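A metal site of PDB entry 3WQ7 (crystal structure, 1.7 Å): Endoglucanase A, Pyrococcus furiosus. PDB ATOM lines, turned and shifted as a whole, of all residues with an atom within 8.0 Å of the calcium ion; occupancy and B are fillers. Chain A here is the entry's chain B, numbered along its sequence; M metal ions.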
ATOM      1  N   PRO A  66      -9.429  15.327   0.020  1.00  0.00           N
ATOM      2  CA  PRO A  66      -8.837  16.210  -0.973  1.00  0.00           C
ATOM      3  C   PRO A  66      -7.593  15.553  -1.610  1.00  0.00           C
ATOM      4  O   PRO A  66      -7.013  14.712  -0.942  1.00  0.00           O
ATOM      5  CB  PRO A  66      -8.436  17.467  -0.098  1.00  0.00           C
ATOM      6  CG  PRO A  66      -8.105  16.905   1.251  1.00  0.00           C
ATOM      7  CD  PRO A  66      -9.067  15.691   1.410  1.00  0.00           C
ATOM      8  N   ILE A  67      -7.306  15.782  -2.888  1.00  0.00           N
ATOM      9  CA  ILE A  67      -6.013  15.316  -3.518  1.00  0.00           C
ATOM     10  C   ILE A  67      -5.223  16.663  -3.468  1.00  0.00           C
ATOM     11  O   ILE A  67      -5.655  17.634  -4.116  1.00  0.00           O
ATOM     12  CB  ILE A  67      -6.266  14.805  -4.929  1.00  0.00           C
ATOM     13  CG1 ILE A  67      -7.085  13.478  -4.818  1.00  0.00           C
ATOM     14  CG2 ILE A  67      -4.945  14.592  -5.690  1.00  0.00           C
ATOM     15  CD1 ILE A  67      -7.565  12.926  -6.155  1.00  0.00           C
ATOM     16  N   ASP A  68      -4.131  16.648  -2.675  1.00  0.00           N
ATOM     17  CA  ASP A  68      -3.210  17.792  -2.387  1.00  0.00           C
ATOM     18  C   ASP A  68      -1.780  17.448  -2.860  1.00  0.00           C
ATOM     19  O   ASP A  68      -0.926  17.298  -1.981  1.00  0.00           O
ATOM     20  CB  ASP A  68      -3.092  17.830  -0.858  1.00  0.00           C
ATOM     21  CG  ASP A  68      -3.390  19.152  -0.241  1.00  0.00           C
ATOM     22  OD1 ASP A  68      -2.587  20.135  -0.429  1.00  0.00           O
ATOM     23  OD2 ASP A  68      -4.395  19.149   0.552  1.00  0.00           O
ATOM     24  N   LYS A  69      -1.532  17.293  -4.166  1.00  0.00           N
ATOM     25  CA  LYS A  69      -0.155  16.986  -4.701  1.00  0.00           C
ATOM     26  C   LYS A  69       1.007  17.905  -4.192  1.00  0.00           C
ATOM     27  O   LYS A  69       2.036  17.418  -3.704  1.00  0.00           O
ATOM     28  CB  LYS A  69      -0.156  16.863  -6.259  1.00  0.00           C
ATOM     29  CG  LYS A  69       1.167  17.098  -7.006  1.00  0.00           C
ATOM     30  CD  LYS A  69       2.231  16.003  -6.830  1.00  0.00           C
ATOM     31  CE  LYS A  69       3.579  16.376  -7.470  1.00  0.00           C
ATOM     32  NZ  LYS A  69       4.503  17.217  -6.634  1.00  0.00           N
ATOM     33  N   ASP A  70       0.858  19.224  -4.329  1.00  0.00           N
ATOM     34  CA  ASP A  70       1.968  20.099  -3.938  1.00  0.00           C
ATOM     35  C   ASP A  70       2.011  20.341  -2.416  1.00  0.00           C
ATOM     36  O   ASP A  70       2.872  21.064  -1.908  1.00  0.00           O
ATOM     37  CB  ASP A  70       1.890  21.437  -4.703  1.00  0.00           C
ATOM     38  CG  ASP A  70       0.737  22.317  -4.218  1.00  0.00           C
ATOM     39  OD1 ASP A  70       0.769  23.540  -4.440  1.00  0.00           O
ATOM     40  OD2 ASP A  70      -0.200  21.773  -3.607  1.00  0.00           O
ATOM     41  N   GLY A  71       1.046  19.736  -1.701  1.00  0.00           N
ATOM     42  CA  GLY A  71       0.885  19.921  -0.257  1.00  0.00           C
ATOM     43  C   GLY A  71       0.789  21.396   0.153  1.00  0.00           C
ATOM     44  O   GLY A  71       1.326  21.773   1.200  1.00  0.00           O
ATOM     45  N   ASP A  72       0.140  22.206  -0.696  1.00  0.00           N
ATOM     46  CA  ASP A  72      -0.089  23.639  -0.463  1.00  0.00           C
ATOM     47  C   ASP A  72      -1.354  23.878   0.376  1.00  0.00           C
ATOM     48  O   ASP A  72      -1.605  25.005   0.835  1.00  0.00           O
ATOM     49  CB  ASP A  72      -0.195  24.408  -1.790  1.00  0.00           C
ATOM     50  CG  ASP A  72      -1.499  24.096  -2.559  1.00  0.00           C
ATOM     51  OD1 ASP A  72      -1.918  24.894  -3.418  1.00  0.00           O
ATOM     52  OD2 ASP A  72      -2.111  23.036  -2.297  1.00  0.00           O
ATOM     53  N   GLY A  73      -2.166  22.820   0.539  1.00  0.00           N
ATOM     54  CA  GLY A  73      -3.341  22.868   1.400  1.00  0.00           C
ATOM     55  C   GLY A  73      -4.617  23.064   0.594  1.00  0.00           C
ATOM     56  O   GLY A  73      -5.686  22.639   1.035  1.00  0.00           O
ATOM     57  N   ASN A  74      -4.511  23.707  -0.570  1.00  0.00           N
ATOM     58  CA  ASN A  74      -5.664  23.871  -1.462  1.00  0.00           C
ATOM     59  C   ASN A  74      -5.737  22.784  -2.564  1.00  0.00           C
ATOM     60  O   ASN A  74      -4.921  22.748  -3.491  1.00  0.00           O
ATOM     61  CB  ASN A  74      -5.693  25.285  -2.088  1.00  0.00           C
ATOM     62  CG  ASN A  74      -6.902  25.522  -2.985  1.00  0.00           C
ATOM     63  OD1 ASN A  74      -7.769  24.651  -3.149  1.00  0.00           O
ATOM     64  ND2 ASN A  74      -6.949  26.704  -3.611  1.00  0.00           N
ATOM     65  N   PRO A  75      -6.734  21.875  -2.463  1.00  0.00           N
ATOM     66  CA  PRO A  75      -6.804  20.692  -3.334  1.00  0.00           C
ATOM     67  C   PRO A  75      -6.925  20.972  -4.864  1.00  0.00           C
ATOM     68  O   PRO A  75      -7.709  21.849  -5.283  1.00  0.00           O
ATOM     69  CB  PRO A  75      -8.103  19.998  -2.824  1.00  0.00           C
ATOM     70  CG  PRO A  75      -8.306  20.462  -1.398  1.00  0.00           C
ATOM     71  CD  PRO A  75      -7.863  21.914  -1.480  1.00  0.00           C
ATOM     72  N   GLU A  76      -6.174  20.227  -5.693  1.00  0.00           N
ATOM     73  CA  GLU A  76      -6.430  20.203  -7.134  1.00  0.00           C
ATOM     74  C   GLU A  76      -7.783  19.544  -7.420  1.00  0.00           C
ATOM     75  O   GLU A  76      -8.449  19.911  -8.364  1.00  0.00           O
ATOM     76  CB  GLU A  76      -5.347  19.470  -7.944  1.00  0.00           C
ATOM     77  CG  GLU A  76      -5.826  18.976  -9.332  1.00  0.00           C
ATOM     78  CD  GLU A  76      -5.809  20.002 -10.463  1.00  0.00           C
ATOM     79  OE1 GLU A  76      -6.777  20.861 -10.611  1.00  0.00           O
ATOM     80  OE2 GLU A  76      -4.841  19.890 -11.261  1.00  0.00           O
ATOM     81  N   PHE A  77      -8.111  18.511  -6.628  1.00  0.00           N
ATOM     82  CA  PHE A  77      -9.342  17.705  -6.815  1.00  0.00           C
ATOM     83  C   PHE A  77      -9.917  17.236  -5.471  1.00  0.00           C
ATOM     84  O   PHE A  77      -9.224  17.237  -4.415  1.00  0.00           O
ATOM     85  CB  PHE A  77      -9.106  16.488  -7.768  1.00  0.00           C
ATOM     86  CG  PHE A  77      -8.798  16.835  -9.207  1.00  0.00           C
ATOM     87  CD1 PHE A  77      -9.791  17.384 -10.084  1.00  0.00           C
ATOM     88  CD2 PHE A  77      -7.489  16.571  -9.748  1.00  0.00           C
ATOM     89  CE1 PHE A  77      -9.475  17.687 -11.433  1.00  0.00           C
ATOM     90  CE2 PHE A  77      -7.210  16.898 -11.097  1.00  0.00           C
ATOM     91  CZ  PHE A  77      -8.189  17.428 -11.926  1.00  0.00           C
ATOM     92  N   ALA A 140     -12.240  22.119  -4.295  1.00  0.00           N
ATOM     93  CA  ALA A 140     -10.844  22.017  -4.814  1.00  0.00           C
ATOM     94  C   ALA A 140     -10.683  23.130  -5.816  1.00  0.00           C
ATOM     95  O   ALA A 140     -11.315  23.105  -6.856  1.00  0.00           O
ATOM     96  CB  ALA A 140     -10.608  20.683  -5.480  1.00  0.00           C
ATOM     97  N   THR A 141      -9.834  24.120  -5.520  1.00  0.00           N
ATOM     98  CA  THR A 141      -9.700  25.211  -6.486  1.00  0.00           C
ATOM     99  C   THR A 141      -8.284  25.522  -6.898  1.00  0.00           C
ATOM    100  O   THR A 141      -7.948  26.668  -7.065  1.00  0.00           O
ATOM    101  CB  THR A 141     -10.463  26.494  -6.031  1.00  0.00           C
ATOM    102  OG1 THR A 141     -10.131  26.819  -4.651  1.00  0.00           O
ATOM    103  CG2 THR A 141     -11.968  26.271  -6.210  1.00  0.00           C
ATOM    104  N   ASP A 142      -7.463  24.477  -7.065  1.00  0.00           N
ATOM    105  CA  ASP A 142      -6.108  24.655  -7.517  1.00  0.00           C
ATOM    106  C   ASP A 142      -5.947  24.134  -8.922  1.00  0.00           C
ATOM    107  O   ASP A 142      -5.480  23.003  -9.115  1.00  0.00           O
ATOM    108  CB  ASP A 142      -5.200  23.877  -6.549  1.00  0.00           C
ATOM    109  CG  ASP A 142      -3.702  24.133  -6.785  1.00  0.00           C
ATOM    110  OD1 ASP A 142      -3.316  24.651  -7.865  1.00  0.00           O
ATOM    111  OD2 ASP A 142      -2.936  23.758  -5.862  1.00  0.00           O
ATOM    112  N   GLY A 143      -6.320  24.952  -9.914  1.00  0.00           N
ATOM    113  CA  GLY A 143      -6.448  24.486 -11.308  1.00  0.00           C
ATOM    114  C   GLY A 143      -6.467  25.745 -12.159  1.00  0.00           C
ATOM    115  O   GLY A 143      -6.626  26.843 -11.589  1.00  0.00           O
HETATM  116 CA    CA M   1      -2.953  21.268  -3.897  1.00  0.00          CA
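N of Asp 142 is in hydrogen-bond range of O of Pro 75.
N of Thr 141 sits at hydrogen-bond distance from OD1 of Asn 74.
N of Asp 72 lies within hydrogen-bond range of OD1 of Asp 68.
The side-chain carboxylate (OD1) of Asp 68 is in hydrogen-bond range of the backbone NH (N) of Gly 73, 2.9 Å away.
The backbone carbonyl oxygen of Pro 75 is in hydrogen-bond range of the backbone NH of Thr 141.
The backbone NH (N) of Glu 76 sits at hydrogen-bond distance from the backbone carbonyl oxygen (O) of Ile 67 (3.1 Å).
Asp 68 touches the calcium ion.
Pro 75 touches the calcium ion.
Glu 76 touches the calcium ion (N to CA, 3.8 Å).
OD2 of Asp 142 touches the calcium ion, 3.2 Å away.
The nearest printed residue that does not touch the calcium ion is Lys 69 (4.2 Å).
The calcium ion is bound by the backbone carbonyl oxygen of Asn 74 (2.5 Å), the side-chain carboxylate of Asp 72 (2.5 Å) and the side-chain carboxylate of Asp 70 (2.8 Å).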
